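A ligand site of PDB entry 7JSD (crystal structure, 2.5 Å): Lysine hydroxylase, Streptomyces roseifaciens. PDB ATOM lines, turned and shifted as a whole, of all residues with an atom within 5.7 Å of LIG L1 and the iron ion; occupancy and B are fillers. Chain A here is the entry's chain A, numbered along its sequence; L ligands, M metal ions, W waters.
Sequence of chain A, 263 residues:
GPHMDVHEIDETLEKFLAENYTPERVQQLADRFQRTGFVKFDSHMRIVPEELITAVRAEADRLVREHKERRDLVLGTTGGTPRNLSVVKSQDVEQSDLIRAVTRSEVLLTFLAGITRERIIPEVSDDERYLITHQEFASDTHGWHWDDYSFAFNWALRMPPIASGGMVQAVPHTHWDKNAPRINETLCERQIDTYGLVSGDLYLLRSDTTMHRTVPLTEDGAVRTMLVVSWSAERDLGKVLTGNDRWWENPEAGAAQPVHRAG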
ATOM      1  N   LEU A  75       7.104  22.177   4.734  1.00  0.00           N
ATOM      2  CA  LEU A  75       8.127  22.316   5.757  1.00  0.00           C
ATOM      3  C   LEU A  75       9.333  23.048   5.175  1.00  0.00           C
ATOM      4  O   LEU A  75       9.955  22.556   4.223  1.00  0.00           O
ATOM      5  CB  LEU A  75       8.542  20.949   6.313  1.00  0.00           C
ATOM      6  CG  LEU A  75       9.253  20.973   7.656  1.00  0.00           C
ATOM      7  CD1 LEU A  75       8.281  21.380   8.760  1.00  0.00           C
ATOM      8  CD2 LEU A  75       9.891  19.633   7.960  1.00  0.00           C
ATOM      9  N   THR A  78      12.859  21.392   4.955  1.00  0.00           N
ATOM     10  CA  THR A  78      13.012  20.360   3.941  1.00  0.00           C
ATOM     11  C   THR A  78      12.630  20.900   2.563  1.00  0.00           C
ATOM     12  O   THR A  78      11.933  20.243   1.794  1.00  0.00           O
ATOM     13  CB  THR A  78      12.186  19.120   4.281  1.00  0.00           C
ATOM     14  OG1 THR A  78      10.833  19.502   4.528  1.00  0.00           O
ATOM     15  CG2 THR A  78      12.755  18.418   5.504  1.00  0.00           C
ATOM     16  N   ARG A  83       3.412  17.997   3.302  1.00  0.00           N
ATOM     17  CA  ARG A  83       2.892  16.949   4.162  1.00  0.00           C
ATOM     18  C   ARG A  83       1.373  16.996   4.040  1.00  0.00           C
ATOM     19  O   ARG A  83       0.736  17.916   4.564  1.00  0.00           O
ATOM     20  CB  ARG A  83       3.327  17.134   5.613  1.00  0.00           C
ATOM     21  CG  ARG A  83       4.812  17.365   5.826  1.00  0.00           C
ATOM     22  CD  ARG A  83       5.641  16.135   5.510  1.00  0.00           C
ATOM     23  NE  ARG A  83       7.039  16.344   5.887  1.00  0.00           N
ATOM     24  CZ  ARG A  83       7.937  16.946   5.107  1.00  0.00           C
ATOM     25  NH1 ARG A  83       7.590  17.400   3.915  1.00  0.00           N
ATOM     26  NH2 ARG A  83       9.181  17.102   5.542  1.00  0.00           N
ATOM     27  N   GLU A 128       8.286  12.298  19.269  1.00  0.00           N
ATOM     28  CA  GLU A 128       8.681  11.579  18.069  1.00  0.00           C
ATOM     29  C   GLU A 128       8.990  10.104  18.341  1.00  0.00           C
ATOM     30  O   GLU A 128       9.575   9.441  17.490  1.00  0.00           O
ATOM     31  CB  GLU A 128       9.894  12.252  17.411  1.00  0.00           C
ATOM     32  CG  GLU A 128      10.013  12.002  15.904  1.00  0.00           C
ATOM     33  CD  GLU A 128      11.281  12.589  15.310  1.00  0.00           C
ATOM     34  OE1 GLU A 128      11.869  13.501  15.936  1.00  0.00           O
ATOM     35  OE2 GLU A 128      11.696  12.140  14.218  1.00  0.00           O
ATOM     36  N   LEU A 131       4.597   7.324  15.691  1.00  0.00           N
ATOM     37  CA  LEU A 131       3.779   8.127  14.803  1.00  0.00           C
ATOM     38  C   LEU A 131       2.992   7.200  13.893  1.00  0.00           C
ATOM     39  O   LEU A 131       3.543   6.219  13.382  1.00  0.00           O
ATOM     40  CB  LEU A 131       4.634   9.090  13.960  1.00  0.00           C
ATOM     41  CG  LEU A 131       3.872  10.123  13.124  1.00  0.00           C
ATOM     42  CD1 LEU A 131       3.295  11.207  14.017  1.00  0.00           C
ATOM     43  CD2 LEU A 131       4.763  10.720  12.045  1.00  0.00           C
ATOM     44  N   HIS A 142       3.797  12.179   1.851  1.00  0.00           N
ATOM     45  CA  HIS A 142       4.761  12.533   2.893  1.00  0.00           C
ATOM     46  C   HIS A 142       6.030  12.931   2.143  1.00  0.00           C
ATOM     47  O   HIS A 142       6.807  12.077   1.726  1.00  0.00           O
ATOM     48  CB  HIS A 142       4.986  11.355   3.842  1.00  0.00           C
ATOM     49  CG  HIS A 142       5.687  11.732   5.117  1.00  0.00           C
ATOM     50  ND1 HIS A 142       5.517  11.023   6.288  1.00  0.00           N
ATOM     51  CD2 HIS A 142       6.548  12.729   5.405  1.00  0.00           C
ATOM     52  CE1 HIS A 142       6.251  11.564   7.239  1.00  0.00           C
ATOM     53  NE2 HIS A 142       6.882  12.610   6.728  1.00  0.00           N
ATOM     54  N   GLY A 143       6.223  14.242   1.976  1.00  0.00           N
ATOM     55  CA  GLY A 143       7.217  14.751   1.061  1.00  0.00           C
ATOM     56  C   GLY A 143       8.644  14.402   1.453  1.00  0.00           C
ATOM     57  O   GLY A 143       8.925  13.850   2.520  1.00  0.00           O
ATOM     58  N   HIS A 145      12.224  14.367   2.835  1.00  0.00           N
ATOM     59  CA  HIS A 145      12.676  14.818   4.150  1.00  0.00           C
ATOM     60  C   HIS A 145      13.757  13.864   4.647  1.00  0.00           C
ATOM     61  O   HIS A 145      14.024  12.819   4.056  1.00  0.00           O
ATOM     62  CB  HIS A 145      11.520  14.870   5.149  1.00  0.00           C
ATOM     63  CG  HIS A 145      11.003  13.518   5.538  1.00  0.00           C
ATOM     64  ND1 HIS A 145      10.018  12.869   4.822  1.00  0.00           N
ATOM     65  CD2 HIS A 145      11.345  12.686   6.545  1.00  0.00           C
ATOM     66  CE1 HIS A 145       9.769  11.695   5.389  1.00  0.00           C
ATOM     67  NE2 HIS A 145      10.558  11.566   6.443  1.00  0.00           N
ATOM     68  N   TRP A 146      14.383  14.261   5.747  1.00  0.00           N
ATOM     69  CA  TRP A 146      15.164  13.379   6.601  1.00  0.00           C
ATOM     70  C   TRP A 146      14.540  13.368   7.992  1.00  0.00           C
ATOM     71  O   TRP A 146      13.667  14.168   8.306  1.00  0.00           O
ATOM     72  CB  TRP A 146      16.637  13.829   6.697  1.00  0.00           C
ATOM     73  CG  TRP A 146      17.377  13.877   5.398  1.00  0.00           C
ATOM     74  CD1 TRP A 146      18.188  12.911   4.874  1.00  0.00           C
ATOM     75  CD2 TRP A 146      17.388  14.972   4.469  1.00  0.00           C
ATOM     76  NE1 TRP A 146      18.697  13.331   3.661  1.00  0.00           N
ATOM     77  CE2 TRP A 146      18.223  14.588   3.391  1.00  0.00           C
ATOM     78  CE3 TRP A 146      16.770  16.222   4.437  1.00  0.00           C
ATOM     79  CZ2 TRP A 146      18.457  15.423   2.302  1.00  0.00           C
ATOM     80  CZ3 TRP A 146      17.005  17.046   3.346  1.00  0.00           C
ATOM     81  CH2 TRP A 146      17.845  16.648   2.297  1.00  0.00           C
ATOM     82  N   ASP A 147      15.011  12.444   8.815  1.00  0.00           N
ATOM     83  CA  ASP A 147      14.602  12.379  10.218  1.00  0.00           C
ATOM     84  C   ASP A 147      15.746  12.866  11.096  1.00  0.00           C
ATOM     85  O   ASP A 147      16.923  12.792  10.722  1.00  0.00           O
ATOM     86  CB  ASP A 147      14.189  10.963  10.616  1.00  0.00           C
ATOM     87  CG  ASP A 147      12.778  10.613  10.164  1.00  0.00           C
ATOM     88  OD1 ASP A 147      12.518  10.632   8.939  1.00  0.00           O
ATOM     89  OD2 ASP A 147      11.937  10.317  11.027  1.00  0.00           O
ATOM     90  N   ASP A 148      15.388  13.367  12.277  1.00  0.00           N
ATOM     91  CA  ASP A 148      16.397  13.842  13.220  1.00  0.00           C
ATOM     92  C   ASP A 148      17.212  12.680  13.792  1.00  0.00           C
ATOM     93  O   ASP A 148      18.369  12.867  14.172  1.00  0.00           O
ATOM     94  CB  ASP A 148      15.741  14.640  14.344  1.00  0.00           C
ATOM     95  CG  ASP A 148      15.044  15.883  13.835  1.00  0.00           C
ATOM     96  OD1 ASP A 148      15.715  16.744  13.228  1.00  0.00           O
ATOM     97  OD2 ASP A 148      13.809  15.999  14.029  1.00  0.00           O
ATOM     98  N   ALA A 152      14.550   4.301  11.728  1.00  0.00           N
ATOM     99  CA  ALA A 152      13.086   4.310  11.688  1.00  0.00           C
ATOM    100  C   ALA A 152      12.619   2.900  11.408  1.00  0.00           C
ATOM    101  O   ALA A 152      13.033   2.283  10.422  1.00  0.00           O
ATOM    102  CB  ALA A 152      12.559   5.277  10.618  1.00  0.00           C
ATOM    103  N   TRP A 176      20.991  15.898   6.223  1.00  0.00           N
ATOM    104  CA  TRP A 176      20.008  16.963   6.395  1.00  0.00           C
ATOM    105  C   TRP A 176      20.730  18.253   6.749  1.00  0.00           C
ATOM    106  O   TRP A 176      21.412  18.339   7.789  1.00  0.00           O
ATOM    107  CB  TRP A 176      19.003  16.590   7.476  1.00  0.00           C
ATOM    108  CG  TRP A 176      17.787  17.485   7.498  1.00  0.00           C
ATOM    109  CD1 TRP A 176      17.553  18.567   6.710  1.00  0.00           C
ATOM    110  CD2 TRP A 176      16.645  17.348   8.346  1.00  0.00           C
ATOM    111  NE1 TRP A 176      16.332  19.125   7.012  1.00  0.00           N
ATOM    112  CE2 TRP A 176      15.751  18.385   8.013  1.00  0.00           C
ATOM    113  CE3 TRP A 176      16.280  16.444   9.347  1.00  0.00           C
ATOM    114  CZ2 TRP A 176      14.530  18.557   8.654  1.00  0.00           C
ATOM    115  CZ3 TRP A 176      15.059  16.616   9.988  1.00  0.00           C
ATOM    116  CH2 TRP A 176      14.200  17.659   9.638  1.00  0.00           C
ATOM    117  N   LEU A 205      14.809   1.714   8.223  1.00  0.00           N
ATOM    118  CA  LEU A 205      15.312   2.840   7.447  1.00  0.00           C
ATOM    119  C   LEU A 205      16.398   3.558   8.233  1.00  0.00           C
ATOM    120  O   LEU A 205      16.224   3.841   9.423  1.00  0.00           O
ATOM    121  CB  LEU A 205      14.189   3.827   7.109  1.00  0.00           C
ATOM    122  CG  LEU A 205      14.572   5.062   6.280  1.00  0.00           C
ATOM    123  CD1 LEU A 205      14.903   4.677   4.845  1.00  0.00           C
ATOM    124  CD2 LEU A 205      13.468   6.094   6.329  1.00  0.00           C
ATOM    125  N   SER A 207      17.205   6.692   8.653  1.00  0.00           N
ATOM    126  CA  SER A 207      16.356   7.827   8.308  1.00  0.00           C
ATOM    127  C   SER A 207      17.061   9.173   8.408  1.00  0.00           C
ATOM    128  O   SER A 207      16.487  10.175   7.958  1.00  0.00           O
ATOM    129  CB  SER A 207      15.122   7.828   9.194  1.00  0.00           C
ATOM    130  OG  SER A 207      15.478   7.856  10.567  1.00  0.00           O
ATOM    131  N   HIS A 212      14.017  10.529   2.001  1.00  0.00           N
ATOM    132  CA  HIS A 212      12.930   9.624   1.643  1.00  0.00           C
ATOM    133  C   HIS A 212      11.602  10.354   1.613  1.00  0.00           C
ATOM    134  O   HIS A 212      11.461  11.471   2.138  1.00  0.00           O
ATOM    135  CB  HIS A 212      12.859   8.435   2.626  1.00  0.00           C
ATOM    136  CG  HIS A 212      12.849   8.847   4.063  1.00  0.00           C
ATOM    137  ND1 HIS A 212      13.974   9.284   4.720  1.00  0.00           N
ATOM    138  CD2 HIS A 212      11.839   8.896   4.968  1.00  0.00           C
ATOM    139  CE1 HIS A 212      13.660   9.575   5.970  1.00  0.00           C
ATOM    140  NE2 HIS A 212      12.369   9.354   6.144  1.00  0.00           N
ATOM    141  N   VAL A 228       5.183   4.476  12.434  1.00  0.00           N
ATOM    142  CA  VAL A 228       6.571   4.902  12.368  1.00  0.00           C
ATOM    143  C   VAL A 228       7.150   4.894  13.773  1.00  0.00           C
ATOM    144  O   VAL A 228       6.654   5.599  14.663  1.00  0.00           O
ATOM    145  CB  VAL A 228       6.714   6.281  11.718  1.00  0.00           C
ATOM    146  CG1 VAL A 228       8.182   6.673  11.598  1.00  0.00           C
ATOM    147  CG2 VAL A 228       6.031   6.295  10.354  1.00  0.00           C
ATOM    148  N   SER A 230      10.711   5.553  15.866  1.00  0.00           N
ATOM    149  CA  SER A 230      12.004   6.202  15.747  1.00  0.00           C
ATOM    150  C   SER A 230      12.917   5.756  16.885  1.00  0.00           C
ATOM    151  O   SER A 230      12.505   5.687  18.043  1.00  0.00           O
ATOM    152  CB  SER A 230      11.861   7.729  15.769  1.00  0.00           C
ATOM    153  OG  SER A 230      11.050   8.173  14.704  1.00  0.00           O
ATOM    154  N   ASP A 245      10.633  22.595  13.466  1.00  0.00           N
ATOM    155  CA  ASP A 245       9.944  21.995  12.330  1.00  0.00           C
ATOM    156  C   ASP A 245       9.238  20.697  12.716  1.00  0.00           C
ATOM    157  O   ASP A 245       9.135  19.774  11.907  1.00  0.00           O
ATOM    158  CB  ASP A 245      10.917  21.745  11.186  1.00  0.00           C
ATOM    159  CG  ASP A 245      12.088  20.864  11.591  1.00  0.00           C
ATOM    160  OD1 ASP A 245      12.466  20.891  12.773  1.00  0.00           O
ATOM    161  OD2 ASP A 245      12.616  20.138  10.716  1.00  0.00           O
ATOM    162  N   TRP A 247       6.277  19.404  12.758  1.00  0.00           N
ATOM    163  CA  TRP A 247       4.943  19.642  12.218  1.00  0.00           C
ATOM    164  C   TRP A 247       3.924  18.627  12.700  1.00  0.00           C
ATOM    165  O   TRP A 247       2.736  18.950  12.826  1.00  0.00           O
ATOM    166  CB  TRP A 247       5.001  19.634  10.689  1.00  0.00           C
ATOM    167  CG  TRP A 247       5.552  18.353  10.146  1.00  0.00           C
ATOM    168  CD1 TRP A 247       6.858  18.046   9.919  1.00  0.00           C
ATOM    169  CD2 TRP A 247       4.801  17.182   9.797  1.00  0.00           C
ATOM    170  NE1 TRP A 247       6.967  16.767   9.438  1.00  0.00           N
ATOM    171  CE2 TRP A 247       5.719  16.213   9.354  1.00  0.00           C
ATOM    172  CE3 TRP A 247       3.436  16.868   9.807  1.00  0.00           C
ATOM    173  CZ2 TRP A 247       5.323  14.954   8.921  1.00  0.00           C
ATOM    174  CZ3 TRP A 247       3.045  15.608   9.383  1.00  0.00           C
ATOM    175  CH2 TRP A 247       3.991  14.672   8.941  1.00  0.00           C
ATOM    176  N   TRP A 248       4.352  17.389  12.950  1.00  0.00           N
ATOM    177  CA  TRP A 248       3.406  16.344  13.337  1.00  0.00           C
ATOM    178  C   TRP A 248       2.839  16.612  14.731  1.00  0.00           C
ATOM    179  O   TRP A 248       1.632  16.493  14.953  1.00  0.00           O
ATOM    180  CB  TRP A 248       4.076  14.971  13.275  1.00  0.00           C
ATOM    181  CG  TRP A 248       5.264  14.828  14.175  1.00  0.00           C
ATOM    182  CD1 TRP A 248       5.283  14.258  15.415  1.00  0.00           C
ATOM    183  CD2 TRP A 248       6.601  15.270  13.913  1.00  0.00           C
ATOM    184  NE1 TRP A 248       6.561  14.312  15.934  1.00  0.00           N
ATOM    185  CE2 TRP A 248       7.384  14.928  15.024  1.00  0.00           C
ATOM    186  CE3 TRP A 248       7.213  15.923  12.831  1.00  0.00           C
ATOM    187  CZ2 TRP A 248       8.741  15.218  15.105  1.00  0.00           C
ATOM    188  CZ3 TRP A 248       8.561  16.212  12.916  1.00  0.00           C
ATOM    189  CH2 TRP A 248       9.318  15.856  14.039  1.00  0.00           C
HETATM  190  N1  LIG L   1      11.268  14.811  10.114  1.00  0.00           N
HETATM  191  C1  LIG L   1      10.136  14.195   9.429  1.00  0.00           C
HETATM  192  C2  LIG L   1       9.499  15.162   8.435  1.00  0.00           C
HETATM  193  O1  LIG L   1       8.570  14.802   7.723  1.00  0.00           O
HETATM  194  C3  LIG L   1       9.083  13.717  10.444  1.00  0.00           C
HETATM  195  C4  LIG L   1       9.479  12.468  11.212  1.00  0.00           C
HETATM  196  C5  LIG L   1       8.350  11.974  12.084  1.00  0.00           C
HETATM  197  C6  LIG L   1       8.522  10.503  12.446  1.00  0.00           C
HETATM  198  N2  LIG L   1       9.833  10.237  13.094  1.00  0.00           N
HETATM  199  O2  LIG L   1       9.901  16.320   8.328  1.00  0.00           O
HETATM  200  C1  LG2 L   2       8.347   9.427   8.700  1.00  0.00           C
HETATM  201  O1  LG2 L   2       7.333   9.307   9.443  1.00  0.00           O
HETATM  202  O2  LG2 L   2       9.325  10.138   9.068  1.00  0.00           O
HETATM  203  C2  LG2 L   2       8.390   8.721   7.350  1.00  0.00           C
HETATM  204  O3  LG2 L   2       9.346   8.827   6.667  1.00  0.00           O
HETATM  205  C3  LG2 L   2       7.190   7.891   6.899  1.00  0.00           C
HETATM  206  C4  LG2 L   2       7.513   7.016   5.684  1.00  0.00           C
HETATM  207  C5  LG2 L   2       6.390   6.041   5.370  1.00  0.00           C
HETATM  208  O4  LG2 L   2       5.203   6.321   5.648  1.00  0.00           O
HETATM  209  O5  LG2 L   2       6.661   4.940   4.816  1.00  0.00           O
HETATM  210 FE    FE M   1      10.933   9.853   7.788  1.00  0.00          FE
HETATM  211  O   HOH W   1      10.830  17.436  10.968  1.00  0.00           O
HETATM  212  O   HOH W   2       8.312   8.418  14.979  1.00  0.00           O
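N2 of LIG L1 lies within salt-bridge range of OE2 of Glu 128 (2.9 Å). OG of Ser 230 lies within hydrogen-bond range of N2 of LIG L1 (2.9 Å). OD2 of Asp 147 is in salt-bridge range of N2 of LIG L1 (3.0 Å). A nitrogen (N1) of LIG L1 sits at hydrogen-bond distance from the backbone carbonyl oxygen of Trp 146, at 3.1 Å. An oxygen (O1) of LIG L1 sits at hydrogen-bond distance from a ring nitrogen (NE2) of His 142 (2.9 Å). The indole nitrogen (NE1) of Trp 247 is in hydrogen-bond range of an oxygen (O1) of LIG L1 (3.1 Å). O1 of LIG L1 lies within salt-bridge range of NE of Arg 83, at 2.8 Å.
Merely in contact with LIG L1: Leu 75 (3.3 Å), Leu 131 (3.8 Å), Val 228 (3.9 Å) and Trp 248 (3.6 Å). Within 4 Å of LIG L1: Leu 75, Arg 83, Glu 128, Leu 131, His 142, His 145, Trp 146, Asp 147, Val 228, Ser 230, Trp 247 and Trp 248.
The iron ion is bound by an oxygen (O2) of LG2 L2, the side-chain carboxylate of Asp 147, an oxygen (O3) of LG2 L2, a ring nitrogen (NE2) of His 145 and a ring nitrogen (NE2) of His 212. The iron ion has five donor atoms within binding distance.
Water W1 lies within hydrogen-bond range of N1 of LIG L1 (2.8 Å) and O of Asp 245 (3.0 Å). Water W2 lies within hydrogen-bond range of the side-chain hydroxyl (OG) of Ser 230 (2.8 Å), the backbone carbonyl oxygen (O) of Glu 128 (3.0 Å), a nitrogen (N2) of LIG L1 (3.0 Å) and the backbone carbonyl oxygen (O) of Val 228 (3.3 Å).
The backbone carbonyl oxygen of Glu 128 sits close to the side-chain hydroxyl of Ser 230, 3.4 Å away. The guanidinium group (NH2) of Arg 83 sits at hydrogen-bond distance from the side-chain hydroxyl (OG1) of Thr 78, 3.1 Å away. The side-chain hydroxyl (OG1) of Thr 78 lies within hydrogen-bond range of the backbone carbonyl oxygen (O) of Leu 75 (3.2 Å). O of Gly 143 sits at hydrogen-bond distance from ND1 of His 145 (2.7 Å). The backbone carbonyl oxygen (O) of Ser 207 sits at hydrogen-bond distance from the backbone NH (N) of Asp 147. N of Val 228 is in hydrogen-bond range of O of Leu 131.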
